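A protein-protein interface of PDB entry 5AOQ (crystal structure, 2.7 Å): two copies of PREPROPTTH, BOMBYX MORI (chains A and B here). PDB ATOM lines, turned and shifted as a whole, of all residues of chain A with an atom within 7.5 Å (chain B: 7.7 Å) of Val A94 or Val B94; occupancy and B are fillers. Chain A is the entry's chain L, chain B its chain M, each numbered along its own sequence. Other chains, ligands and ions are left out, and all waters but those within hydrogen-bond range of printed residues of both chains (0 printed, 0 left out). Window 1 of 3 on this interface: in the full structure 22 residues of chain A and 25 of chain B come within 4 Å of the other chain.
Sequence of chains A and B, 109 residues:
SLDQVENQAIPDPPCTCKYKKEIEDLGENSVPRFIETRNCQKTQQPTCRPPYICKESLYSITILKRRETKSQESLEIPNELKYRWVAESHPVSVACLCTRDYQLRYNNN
The backbone carbonyl oxygen (O) of Glu A36 is in hydrogen-bond range of the side-chain hydroxyl (OH) of Tyr B59 (2.6 Å).
The guanidinium group (NH1) of Arg A38 sits at hydrogen-bond distance from the side-chain hydroxyl (OG) of Ser B57.
O of Leu B58 sits at hydrogen-bond distance from NH2 of Arg A38 (3.0 Å).
OG of Ser A57 sits at hydrogen-bond distance from NH1 of Arg B38, at 2.9 Å.
O of Leu A58 is in hydrogen-bond range of NH2 of Arg B38 (3.0 Å).
O of Glu B36 lies within hydrogen-bond range of OH of Tyr A59, at 2.6 Å.
The backbone carbonyl oxygen (O) of Arg A38 is in hydrogen-bond range of the backbone NH (N) of Ala A95 (3.5 Å).
The backbone NH (N) of Ser A57 lies within hydrogen-bond range of the backbone carbonyl oxygen (O) of Ala A95, 2.8 Å away.
The backbone carbonyl oxygen of Tyr A59 lies within hydrogen-bond range of the backbone NH of Val A92.
O of Ser B93 is in hydrogen-bond range of N of Arg B38, at 2.9 Å.
The backbone NH of Val B94 sits at hydrogen-bond distance from the backbone carbonyl oxygen of Ser B57, at 2.7 Å.
The backbone NH (N) of Ser B57 lies within hydrogen-bond range of the backbone carbonyl oxygen (O) of Ala B95 (2.6 Å).
CD1 of Tyr B59 touches CZ of Arg A38, 3.7 Å away.
Arg B38 touches Tyr A59.
Val B94 touches Tyr A59 (CG2 to CD1, 3.4 Å).
Val A94 touches Tyr B59.
Val A94 touches Val B94 (CG1 to CG2, 3.4 Å).
CB of Ala A95 touches CB of Ala B95, 3.8 Å away.
CD2 of Leu A97 touches CD2 of Leu B97, 3.8 Å away.
Tyr A19 touches none of the printed residues of chain B.
Of the printed residues of chain B, Glu A36 touches Tyr B59 (2.6 Å).
No residue of chain B comes within 4 Å of Ser A93.
Of chain B, only Tyr B59 and Val B94 come within 4 Å of Val A94.
Of the printed residues of chain B, Leu A97 touches Leu B97.
Of the printed residues of chain A, Arg B38 touches Ser A57 (2.9 Å), Leu A58 (3.0 Å) and Tyr A59 (3.6 Å).
Printed residues of chain A within 4 Å of Tyr B59: Glu A36, Arg A38 and Val A94.
Of the printed residues of chain A, Leu B97 touches Leu A97 (3.8 Å).
The nearest residue of chain B that does not touch Val A94 is Arg B38 (4.4 Å).
The nearest residue of chain A that does not touch Val B94 is Arg A38 (4.4 Å).
Printed residues of chain B that touch a printed residue of chain A: Glu B36, Arg B38, Ser B57, Leu B58, Tyr B59, Val B94, Ala B95 and Leu B97.
Of the 18 printed residues of chain A, 8 touch a printed residue of chain B.
Hydrophobic or aromatic side chains of chain A that line the printed part of chain B: Tyr A59, Val A94, Ala A95 and Leu A97.
Among the printed residues, 13 pairs touch across the chains.
Glu A36 touches Tyr B59, and with the chains exchanged Tyr A59 touches Glu B36.
Arg A38 touches Tyr B59, and with the chains exchanged Tyr A59 touches Arg B38.
Val A94 touches its own counterpart, Val B94.
Ala A95 touches its own counterpart, Ala B95.
Of the 13 pairs that touch across the chains among the printed residues, 13 have their exchanged pair printed and touching as well.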
ATOM      1  N   TYR A  19       4.424  25.646  -4.008  1.00  0.00           N
ATOM      2  CA  TYR A  19       4.092  24.524  -3.131  1.00  0.00           C
ATOM      3  C   TYR A  19       5.233  24.160  -2.180  1.00  0.00           C
ATOM      4  O   TYR A  19       6.396  24.474  -2.437  1.00  0.00           O
ATOM      5  CB  TYR A  19       3.701  23.303  -3.974  1.00  0.00           C
ATOM      6  CG  TYR A  19       4.807  22.752  -4.846  1.00  0.00           C
ATOM      7  CD1 TYR A  19       5.686  21.794  -4.359  1.00  0.00           C
ATOM      8  CD2 TYR A  19       4.961  23.175  -6.158  1.00  0.00           C
ATOM      9  CE1 TYR A  19       6.693  21.282  -5.150  1.00  0.00           C
ATOM     10  CE2 TYR A  19       5.967  22.667  -6.959  1.00  0.00           C
ATOM     11  CZ  TYR A  19       6.829  21.720  -6.449  1.00  0.00           C
ATOM     12  OH  TYR A  19       7.833  21.210  -7.240  1.00  0.00           O
ATOM     13  N   GLU A  36       6.589  11.366  -0.317  1.00  0.00           N
ATOM     14  CA  GLU A  36       6.723  12.776  -0.670  1.00  0.00           C
ATOM     15  C   GLU A  36       5.355  13.432  -0.829  1.00  0.00           C
ATOM     16  O   GLU A  36       4.534  12.984  -1.631  1.00  0.00           O
ATOM     17  CB  GLU A  36       7.531  12.922  -1.964  1.00  0.00           C
ATOM     18  CG  GLU A  36       7.734  14.356  -2.428  1.00  0.00           C
ATOM     19  CD  GLU A  36       8.578  14.445  -3.688  1.00  0.00           C
ATOM     20  OE1 GLU A  36       9.240  13.445  -4.037  1.00  0.00           O
ATOM     21  OE2 GLU A  36       8.572  15.514  -4.334  1.00  0.00           O
ATOM     22  N   THR A  37       5.123  14.492  -0.059  1.00  0.00           N
ATOM     23  CA  THR A  37       3.857  15.221  -0.089  1.00  0.00           C
ATOM     24  C   THR A  37       4.097  16.691  -0.415  1.00  0.00           C
ATOM     25  O   THR A  37       4.833  17.381   0.291  1.00  0.00           O
ATOM     26  CB  THR A  37       3.109  15.113   1.254  1.00  0.00           C
ATOM     27  OG1 THR A  37       2.902  13.733   1.580  1.00  0.00           O
ATOM     28  CG2 THR A  37       1.760  15.823   1.182  1.00  0.00           C
ATOM     29  N   ARG A  38       3.460  17.160  -1.484  1.00  0.00           N
ATOM     30  CA  ARG A  38       3.613  18.536  -1.943  1.00  0.00           C
ATOM     31  C   ARG A  38       2.370  19.364  -1.627  1.00  0.00           C
ATOM     32  O   ARG A  38       1.403  19.367  -2.389  1.00  0.00           O
ATOM     33  CB  ARG A  38       3.899  18.557  -3.446  1.00  0.00           C
ATOM     34  CG  ARG A  38       5.158  17.799  -3.833  1.00  0.00           C
ATOM     35  CD  ARG A  38       5.280  17.635  -5.335  1.00  0.00           C
ATOM     36  NE  ARG A  38       6.471  16.876  -5.708  1.00  0.00           N
ATOM     37  CZ  ARG A  38       6.761  16.500  -6.950  1.00  0.00           C
ATOM     38  NH1 ARG A  38       5.948  16.813  -7.950  1.00  0.00           N
ATOM     39  NH2 ARG A  38       7.866  15.811  -7.193  1.00  0.00           N
ATOM     40  N   ASN A  39       2.409  20.069  -0.501  1.00  0.00           N
ATOM     41  CA  ASN A  39       1.279  20.875  -0.050  1.00  0.00           C
ATOM     42  C   ASN A  39       1.322  22.290  -0.619  1.00  0.00           C
ATOM     43  O   ASN A  39       2.256  22.652  -1.327  1.00  0.00           O
ATOM     44  CB  ASN A  39       1.251  20.928   1.477  1.00  0.00           C
ATOM     45  CG  ASN A  39       1.205  19.549   2.102  1.00  0.00           C
ATOM     46  OD1 ASN A  39       2.109  19.159   2.841  1.00  0.00           O
ATOM     47  ND2 ASN A  39       0.150  18.800   1.805  1.00  0.00           N
ATOM     48  N   GLU A  56      -5.201  22.081  -3.221  1.00  0.00           N
ATOM     49  CA  GLU A  56      -4.200  21.014  -3.212  1.00  0.00           C
ATOM     50  C   GLU A  56      -4.662  19.796  -4.014  1.00  0.00           C
ATOM     51  O   GLU A  56      -5.721  19.225  -3.754  1.00  0.00           O
ATOM     52  CB  GLU A  56      -3.864  20.603  -1.771  1.00  0.00           C
ATOM     53  CG  GLU A  56      -5.017  19.992  -0.981  1.00  0.00           C
ATOM     54  CD  GLU A  56      -4.615  19.598   0.427  1.00  0.00           C
ATOM     55  OE1 GLU A  56      -3.402  19.617   0.730  1.00  0.00           O
ATOM     56  OE2 GLU A  56      -5.511  19.265   1.231  1.00  0.00           O
ATOM     57  N   SER A  57      -3.871  19.427  -5.016  1.00  0.00           N
ATOM     58  CA  SER A  57      -4.210  18.314  -5.894  1.00  0.00           C
ATOM     59  C   SER A  57      -3.938  16.978  -5.214  1.00  0.00           C
ATOM     60  O   SER A  57      -2.785  16.578  -5.052  1.00  0.00           O
ATOM     61  CB  SER A  57      -3.420  18.400  -7.201  1.00  0.00           C
ATOM     62  OG  SER A  57      -3.807  17.374  -8.098  1.00  0.00           O
ATOM     63  N   LEU A  58      -5.003  16.291  -4.815  1.00  0.00           N
ATOM     64  CA  LEU A  58      -4.871  14.986  -4.180  1.00  0.00           C
ATOM     65  C   LEU A  58      -4.606  13.909  -5.223  1.00  0.00           C
ATOM     66  O   LEU A  58      -5.278  13.846  -6.253  1.00  0.00           O
ATOM     67  CB  LEU A  58      -6.125  14.645  -3.374  1.00  0.00           C
ATOM     68  CG  LEU A  58      -6.413  15.552  -2.176  1.00  0.00           C
ATOM     69  CD1 LEU A  58      -7.757  15.203  -1.561  1.00  0.00           C
ATOM     70  CD2 LEU A  58      -5.306  15.447  -1.134  1.00  0.00           C
ATOM     71  N   TYR A  59      -3.620  13.064  -4.939  1.00  0.00           N
ATOM     72  CA  TYR A  59      -3.255  11.965  -5.822  1.00  0.00           C
ATOM     73  C   TYR A  59      -3.141  10.684  -5.009  1.00  0.00           C
ATOM     74  O   TYR A  59      -2.475  10.652  -3.972  1.00  0.00           O
ATOM     75  CB  TYR A  59      -1.937  12.268  -6.538  1.00  0.00           C
ATOM     76  CG  TYR A  59      -1.477  11.179  -7.477  1.00  0.00           C
ATOM     77  CD1 TYR A  59      -1.892  11.155  -8.801  1.00  0.00           C
ATOM     78  CD2 TYR A  59      -0.623  10.176  -7.041  1.00  0.00           C
ATOM     79  CE1 TYR A  59      -1.470  10.162  -9.665  1.00  0.00           C
ATOM     80  CE2 TYR A  59      -0.196   9.179  -7.896  1.00  0.00           C
ATOM     81  CZ  TYR A  59      -0.622   9.177  -9.206  1.00  0.00           C
ATOM     82  OH  TYR A  59      -0.199   8.184 -10.059  1.00  0.00           O
ATOM     83  N   SER A  60      -3.799   9.631  -5.484  1.00  0.00           N
ATOM     84  CA  SER A  60      -3.846   8.366  -4.761  1.00  0.00           C
ATOM     85  C   SER A  60      -2.660   7.478  -5.110  1.00  0.00           C
ATOM     86  O   SER A  60      -2.451   7.130  -6.273  1.00  0.00           O
ATOM     87  CB  SER A  60      -5.156   7.635  -5.059  1.00  0.00           C
ATOM     88  OG  SER A  60      -6.263   8.344  -4.529  1.00  0.00           O
ATOM     89  N   ILE A  61      -1.889   7.118  -4.087  1.00  0.00           N
ATOM     90  CA  ILE A  61      -0.783   6.182  -4.245  1.00  0.00           C
ATOM     91  C   ILE A  61      -1.034   4.932  -3.413  1.00  0.00           C
ATOM     92  O   ILE A  61      -1.801   4.955  -2.448  1.00  0.00           O
ATOM     93  CB  ILE A  61       0.567   6.807  -3.835  1.00  0.00           C
ATOM     94  CG1 ILE A  61       0.498   7.347  -2.403  1.00  0.00           C
ATOM     95  CG2 ILE A  61       0.945   7.917  -4.806  1.00  0.00           C
ATOM     96  CD1 ILE A  61       1.837   7.777  -1.839  1.00  0.00           C
ATOM     97  N   PRO A  91      -4.387   8.674  -0.577  1.00  0.00           N
ATOM     98  CA  PRO A  91      -4.393   9.969  -1.265  1.00  0.00           C
ATOM     99  C   PRO A  91      -3.447  10.955  -0.593  1.00  0.00           C
ATOM    100  O   PRO A  91      -3.432  11.041   0.635  1.00  0.00           O
ATOM    101  CB  PRO A  91      -5.849  10.421  -1.150  1.00  0.00           C
ATOM    102  CG  PRO A  91      -6.351   9.754   0.078  1.00  0.00           C
ATOM    103  CD  PRO A  91      -5.648   8.429   0.145  1.00  0.00           C
ATOM    104  N   VAL A  92      -2.668  11.681  -1.388  1.00  0.00           N
ATOM    105  CA  VAL A  92      -1.738  12.669  -0.852  1.00  0.00           C
ATOM    106  C   VAL A  92      -1.639  13.892  -1.754  1.00  0.00           C
ATOM    107  O   VAL A  92      -1.775  13.792  -2.973  1.00  0.00           O
ATOM    108  CB  VAL A  92      -0.327  12.070  -0.666  1.00  0.00           C
ATOM    109  CG1 VAL A  92      -0.307  11.102   0.508  1.00  0.00           C
ATOM    110  CG2 VAL A  92       0.138  11.381  -1.944  1.00  0.00           C
ATOM    111  N   SER A  93      -1.408  15.050  -1.143  1.00  0.00           N
ATOM    112  CA  SER A  93      -1.183  16.273  -1.897  1.00  0.00           C
ATOM    113  C   SER A  93       0.102  16.127  -2.699  1.00  0.00           C
ATOM    114  O   SER A  93       1.136  15.734  -2.159  1.00  0.00           O
ATOM    115  CB  SER A  93      -1.104  17.483  -0.966  1.00  0.00           C
ATOM    116  OG  SER A  93      -0.952  18.686  -1.703  1.00  0.00           O
ATOM    117  N   VAL A  94       0.029  16.443  -3.988  1.00  0.00           N
ATOM    118  CA  VAL A  94       1.158  16.260  -4.894  1.00  0.00           C
ATOM    119  C   VAL A  94       1.368  17.491  -5.776  1.00  0.00           C
ATOM    120  O   VAL A  94       2.292  17.540  -6.588  1.00  0.00           O
ATOM    121  CB  VAL A  94       0.946  15.006  -5.769  1.00  0.00           C
ATOM    122  CG1 VAL A  94      -0.064  15.281  -6.880  1.00  0.00           C
ATOM    123  CG2 VAL A  94       2.274  14.505  -6.329  1.00  0.00           C
ATOM    124  N   ALA A  95       0.505  18.486  -5.610  1.00  0.00           N
ATOM    125  CA  ALA A  95       0.638  19.743  -6.329  1.00  0.00           C
ATOM    126  C   ALA A  95      -0.326  20.758  -5.741  1.00  0.00           C
ATOM    127  O   ALA A  95      -1.277  20.390  -5.050  1.00  0.00           O
ATOM    128  CB  ALA A  95       0.371  19.551  -7.815  1.00  0.00           C
ATOM    129  N   CYS A  96      -0.074  22.033  -6.014  1.00  0.00           N
ATOM    130  CA  CYS A  96      -0.986  23.096  -5.613  1.00  0.00           C
ATOM    131  C   CYS A  96      -1.507  23.814  -6.847  1.00  0.00           C
ATOM    132  O   CYS A  96      -0.860  24.717  -7.380  1.00  0.00           O
ATOM    133  CB  CYS A  96      -0.302  24.085  -4.670  1.00  0.00           C
ATOM    134  SG  CYS A  96      -1.462  25.232  -3.889  1.00  0.00           S
ATOM    135  N   LEU A  97      -2.684  23.397  -7.301  1.00  0.00           N
ATOM    136  CA  LEU A  97      -3.296  23.965  -8.491  1.00  0.00           C
ATOM    137  C   LEU A  97      -4.069  25.227  -8.137  1.00  0.00           C
ATOM    138  O   LEU A  97      -4.376  25.469  -6.970  1.00  0.00           O
ATOM    139  CB  LEU A  97      -4.223  22.946  -9.155  1.00  0.00           C
ATOM    140  CG  LEU A  97      -3.609  21.566  -9.402  1.00  0.00           C
ATOM    141  CD1 LEU A  97      -4.642  20.626 -10.004  1.00  0.00           C
ATOM    142  CD2 LEU A  97      -2.381  21.662 -10.294  1.00  0.00           C
ATOM    143  N   TYR B  19      -4.710  19.689 -18.269  1.00  0.00           N
ATOM    144  CA  TYR B  19      -4.058  18.444 -17.887  1.00  0.00           C
ATOM    145  C   TYR B  19      -4.962  17.269 -18.247  1.00  0.00           C
ATOM    146  O   TYR B  19      -6.162  17.286 -17.964  1.00  0.00           O
ATOM    147  CB  TYR B  19      -3.719  18.442 -16.392  1.00  0.00           C
ATOM    148  CG  TYR B  19      -4.899  18.179 -15.485  1.00  0.00           C
ATOM    149  CD1 TYR B  19      -5.914  19.116 -15.341  1.00  0.00           C
ATOM    150  CD2 TYR B  19      -4.995  16.994 -14.769  1.00  0.00           C
ATOM    151  CE1 TYR B  19      -6.993  18.876 -14.513  1.00  0.00           C
ATOM    152  CE2 TYR B  19      -6.068  16.746 -13.937  1.00  0.00           C
ATOM    153  CZ  TYR B  19      -7.065  17.691 -13.813  1.00  0.00           C
ATOM    154  OH  TYR B  19      -8.136  17.448 -12.984  1.00  0.00           O
ATOM    155  N   LYS B  21      -5.598  13.034 -18.178  1.00  0.00           N
ATOM    156  CA  LYS B  21      -5.291  11.798 -17.468  1.00  0.00           C
ATOM    157  C   LYS B  21      -5.138  10.607 -18.404  1.00  0.00           C
ATOM    158  O   LYS B  21      -5.818  10.506 -19.426  1.00  0.00           O
ATOM    159  CB  LYS B  21      -6.379  11.497 -16.436  1.00  0.00           C
ATOM    160  CG  LYS B  21      -6.267  12.324 -15.169  1.00  0.00           C
ATOM    161  CD  LYS B  21      -7.360  11.973 -14.179  1.00  0.00           C
ATOM    162  CE  LYS B  21      -7.268  12.816 -12.917  1.00  0.00           C
ATOM    163  NZ  LYS B  21      -8.298  12.438 -11.909  1.00  0.00           N
ATOM    164  N   GLU B  36      -1.763   6.001 -12.448  1.00  0.00           N
ATOM    165  CA  GLU B  36      -2.422   7.221 -12.900  1.00  0.00           C
ATOM    166  C   GLU B  36      -1.394   8.244 -13.376  1.00  0.00           C
ATOM    167  O   GLU B  36      -0.494   8.623 -12.625  1.00  0.00           O
ATOM    168  CB  GLU B  36      -3.279   7.808 -11.775  1.00  0.00           C
ATOM    169  CG  GLU B  36      -4.013   9.088 -12.145  1.00  0.00           C
ATOM    170  CD  GLU B  36      -4.893   9.599 -11.020  1.00  0.00           C
ATOM    171  OE1 GLU B  36      -5.162   8.831 -10.074  1.00  0.00           O
ATOM    172  OE2 GLU B  36      -5.315  10.772 -11.080  1.00  0.00           O
ATOM    173  N   THR B  37      -1.532   8.682 -14.625  1.00  0.00           N
ATOM    174  CA  THR B  37      -0.615   9.655 -15.216  1.00  0.00           C
ATOM    175  C   THR B  37      -1.369  10.887 -15.710  1.00  0.00           C
ATOM    176  O   THR B  37      -2.257  10.778 -16.552  1.00  0.00           O
ATOM    177  CB  THR B  37       0.172   9.039 -16.392  1.00  0.00           C
ATOM    178  OG1 THR B  37       0.871   7.872 -15.945  1.00  0.00           O
ATOM    179  CG2 THR B  37       1.171  10.039 -16.965  1.00  0.00           C
ATOM    180  N   ARG B  38      -0.997  12.055 -15.189  1.00  0.00           N
ATOM    181  CA  ARG B  38      -1.640  13.315 -15.561  1.00  0.00           C
ATOM    182  C   ARG B  38      -0.724  14.153 -16.446  1.00  0.00           C
ATOM    183  O   ARG B  38       0.103  14.915 -15.947  1.00  0.00           O
ATOM    184  CB  ARG B  38      -2.025  14.106 -14.309  1.00  0.00           C
ATOM    185  CG  ARG B  38      -2.979  13.370 -13.384  1.00  0.00           C
ATOM    186  CD  ARG B  38      -3.133  14.087 -12.055  1.00  0.00           C
ATOM    187  NE  ARG B  38      -4.011  13.363 -11.140  1.00  0.00           N
ATOM    188  CZ  ARG B  38      -4.229  13.712  -9.876  1.00  0.00           C
ATOM    189  NH1 ARG B  38      -3.633  14.782  -9.363  1.00  0.00           N
ATOM    190  NH2 ARG B  38      -5.042  12.989  -9.120  1.00  0.00           N
ATOM    191  N   ASN B  39      -0.890  14.025 -17.759  1.00  0.00           N
ATOM    192  CA  ASN B  39      -0.050  14.745 -18.712  1.00  0.00           C
ATOM    193  C   ASN B  39      -0.640  16.110 -19.047  1.00  0.00           C
ATOM    194  O   ASN B  39      -1.677  16.491 -18.507  1.00  0.00           O
ATOM    195  CB  ASN B  39       0.132  13.925 -19.990  1.00  0.00           C
ATOM    196  CG  ASN B  39       0.705  12.549 -19.721  1.00  0.00           C
ATOM    197  OD1 ASN B  39       0.072  11.533 -20.009  1.00  0.00           O
ATOM    198  ND2 ASN B  39       1.911  12.509 -19.165  1.00  0.00           N
ATOM    199  N   GLU B  56       5.169  19.292 -17.254  1.00  0.00           N
ATOM    200  CA  GLU B  56       4.500  18.144 -16.672  1.00  0.00           C
ATOM    201  C   GLU B  56       5.213  17.865 -15.353  1.00  0.00           C
ATOM    202  O   GLU B  56       6.425  17.649 -15.322  1.00  0.00           O
ATOM    203  CB  GLU B  56       4.520  16.939 -17.619  1.00  0.00           C
ATOM    204  CG  GLU B  56       5.888  16.361 -17.935  1.00  0.00           C
ATOM    205  CD  GLU B  56       5.806  15.173 -18.876  1.00  0.00           C
ATOM    206  OE1 GLU B  56       4.682  14.687 -19.125  1.00  0.00           O
ATOM    207  OE2 GLU B  56       6.863  14.724 -19.364  1.00  0.00           O
ATOM    208  N   SER B  57       4.463  17.906 -14.259  1.00  0.00           N
ATOM    209  CA  SER B  57       5.048  17.762 -12.932  1.00  0.00           C
ATOM    210  C   SER B  57       5.422  16.312 -12.661  1.00  0.00           C
ATOM    211  O   SER B  57       4.557  15.468 -12.438  1.00  0.00           O
ATOM    212  CB  SER B  57       4.080  18.267 -11.863  1.00  0.00           C
ATOM    213  OG  SER B  57       4.672  18.222 -10.577  1.00  0.00           O
ATOM    214  N   LEU B  58       6.720  16.032 -12.683  1.00  0.00           N
ATOM    215  CA  LEU B  58       7.213  14.685 -12.438  1.00  0.00           C
ATOM    216  C   LEU B  58       7.209  14.349 -10.952  1.00  0.00           C
ATOM    217  O   LEU B  58       7.681  15.130 -10.124  1.00  0.00           O
ATOM    218  CB  LEU B  58       8.628  14.525 -12.997  1.00  0.00           C
ATOM    219  CG  LEU B  58       8.784  14.657 -14.513  1.00  0.00           C
ATOM    220  CD1 LEU B  58      10.255  14.624 -14.892  1.00  0.00           C
ATOM    221  CD2 LEU B  58       8.015  13.563 -15.244  1.00  0.00           C
ATOM    222  N   TYR B  59       6.666  13.179 -10.628  1.00  0.00           N
ATOM    223  CA  TYR B  59       6.634  12.685  -9.257  1.00  0.00           C
ATOM    224  C   TYR B  59       7.082  11.230  -9.230  1.00  0.00           C
ATOM    225  O   TYR B  59       6.597  10.410 -10.012  1.00  0.00           O
ATOM    226  CB  TYR B  59       5.233  12.827  -8.660  1.00  0.00           C
ATOM    227  CG  TYR B  59       5.124  12.335  -7.235  1.00  0.00           C
ATOM    228  CD1 TYR B  59       5.398  13.178  -6.165  1.00  0.00           C
ATOM    229  CD2 TYR B  59       4.743  11.029  -6.956  1.00  0.00           C
ATOM    230  CE1 TYR B  59       5.301  12.732  -4.860  1.00  0.00           C
ATOM    231  CE2 TYR B  59       4.642  10.574  -5.656  1.00  0.00           C
ATOM    232  CZ  TYR B  59       4.921  11.430  -4.611  1.00  0.00           C
ATOM    233  OH  TYR B  59       4.821  10.981  -3.315  1.00  0.00           O
ATOM    234  N   SER B  60       8.012  10.918  -8.332  1.00  0.00           N
ATOM    235  CA  SER B  60       8.584   9.578  -8.241  1.00  0.00           C
ATOM    236  C   SER B  60       7.762   8.661  -7.343  1.00  0.00           C
ATOM    237  O   SER B  60       7.547   8.961  -6.168  1.00  0.00           O
ATOM    238  CB  SER B  60      10.023   9.646  -7.723  1.00  0.00           C
ATOM    239  OG  SER B  60      10.875  10.280  -8.659  1.00  0.00           O
ATOM    240  N   ILE B  61       7.308   7.546  -7.909  1.00  0.00           N
ATOM    241  CA  ILE B  61       6.610   6.513  -7.149  1.00  0.00           C
ATOM    242  C   ILE B  61       7.421   5.222  -7.183  1.00  0.00           C
ATOM    243  O   ILE B  61       8.254   5.027  -8.071  1.00  0.00           O
ATOM    244  CB  ILE B  61       5.191   6.250  -7.693  1.00  0.00           C
ATOM    245  CG1 ILE B  61       5.242   5.906  -9.184  1.00  0.00           C
ATOM    246  CG2 ILE B  61       4.307   7.467  -7.455  1.00  0.00           C
ATOM    247  CD1 ILE B  61       3.924   5.419  -9.749  1.00  0.00           C
ATOM    248  N   PRO B  91       9.423   8.001 -11.975  1.00  0.00           N
ATOM    249  CA  PRO B  91       8.855   9.342 -12.130  1.00  0.00           C
ATOM    250  C   PRO B  91       7.683   9.340 -13.100  1.00  0.00           C
ATOM    251  O   PRO B  91       7.760   8.694 -14.146  1.00  0.00           O
ATOM    252  CB  PRO B  91      10.026  10.158 -12.678  1.00  0.00           C
ATOM    253  CG  PRO B  91      10.868   9.168 -13.391  1.00  0.00           C
ATOM    254  CD  PRO B  91      10.746   7.888 -12.616  1.00  0.00           C
ATOM    255  N   VAL B  92       6.612  10.041 -12.747  1.00  0.00           N
ATOM    256  CA  VAL B  92       5.443  10.130 -13.613  1.00  0.00           C
ATOM    257  C   VAL B  92       4.821  11.520 -13.531  1.00  0.00           C
ATOM    258  O   VAL B  92       4.876  12.177 -12.491  1.00  0.00           O
ATOM    259  CB  VAL B  92       4.391   9.056 -13.239  1.00  0.00           C
ATOM    260  CG1 VAL B  92       3.873   9.272 -11.819  1.00  0.00           C
ATOM    261  CG2 VAL B  92       3.244   9.045 -14.241  1.00  0.00           C
ATOM    262  N   SER B  93       4.237  11.966 -14.639  1.00  0.00           N
ATOM    263  CA  SER B  93       3.522  13.234 -14.664  1.00  0.00           C
ATOM    264  C   SER B  93       2.322  13.163 -13.733  1.00  0.00           C
ATOM    265  O   SER B  93       1.541  12.215 -13.793  1.00  0.00           O
ATOM    266  CB  SER B  93       3.069  13.578 -16.082  1.00  0.00           C
ATOM    267  OG  SER B  93       2.414  14.834 -16.113  1.00  0.00           O
ATOM    268  N   VAL B  94       2.184  14.169 -12.875  1.00  0.00           N
ATOM    269  CA  VAL B  94       1.127  14.175 -11.872  1.00  0.00           C
ATOM    270  C   VAL B  94       0.422  15.534 -11.821  1.00  0.00           C
ATOM    271  O   VAL B  94      -0.515  15.734 -11.048  1.00  0.00           O
ATOM    272  CB  VAL B  94       1.697  13.814 -10.481  1.00  0.00           C
ATOM    273  CG1 VAL B  94       2.416  15.007  -9.847  1.00  0.00           C
ATOM    274  CG2 VAL B  94       0.596  13.295  -9.577  1.00  0.00           C
ATOM    275  N   ALA B  95       0.877  16.467 -12.651  1.00  0.00           N
ATOM    276  CA  ALA B  95       0.241  17.772 -12.762  1.00  0.00           C
ATOM    277  C   ALA B  95       0.808  18.506 -13.966  1.00  0.00           C
ATOM    278  O   ALA B  95       1.877  18.151 -14.464  1.00  0.00           O
ATOM    279  CB  ALA B  95       0.449  18.588 -11.491  1.00  0.00           C
ATOM    280  N   CYS B  96       0.083  19.516 -14.437  1.00  0.00           N
ATOM    281  CA  CYS B  96       0.567  20.376 -15.511  1.00  0.00           C
ATOM    282  C   CYS B  96       0.653  21.811 -15.000  1.00  0.00           C
ATOM    283  O   CYS B  96      -0.360  22.404 -14.627  1.00  0.00           O
ATOM    284  CB  CYS B  96      -0.341  20.289 -16.738  1.00  0.00           C
ATOM    285  SG  CYS B  96       0.378  21.047 -18.215  1.00  0.00           S
ATOM    286  N   LEU B  97       1.866  22.360 -14.984  1.00  0.00           N
ATOM    287  CA  LEU B  97       2.124  23.655 -14.360  1.00  0.00           C
ATOM    288  C   LEU B  97       2.884  24.588 -15.304  1.00  0.00           C
ATOM    289  O   LEU B  97       3.674  24.137 -16.128  1.00  0.00           O
ATOM    290  CB  LEU B  97       2.902  23.450 -13.060  1.00  0.00           C
ATOM    291  CG  LEU B  97       2.240  22.479 -12.073  1.00  0.00           C
ATOM    292  CD1 LEU B  97       3.165  22.133 -10.912  1.00  0.00           C
ATOM    293  CD2 LEU B  97       0.934  23.053 -11.550  1.00  0.00           C
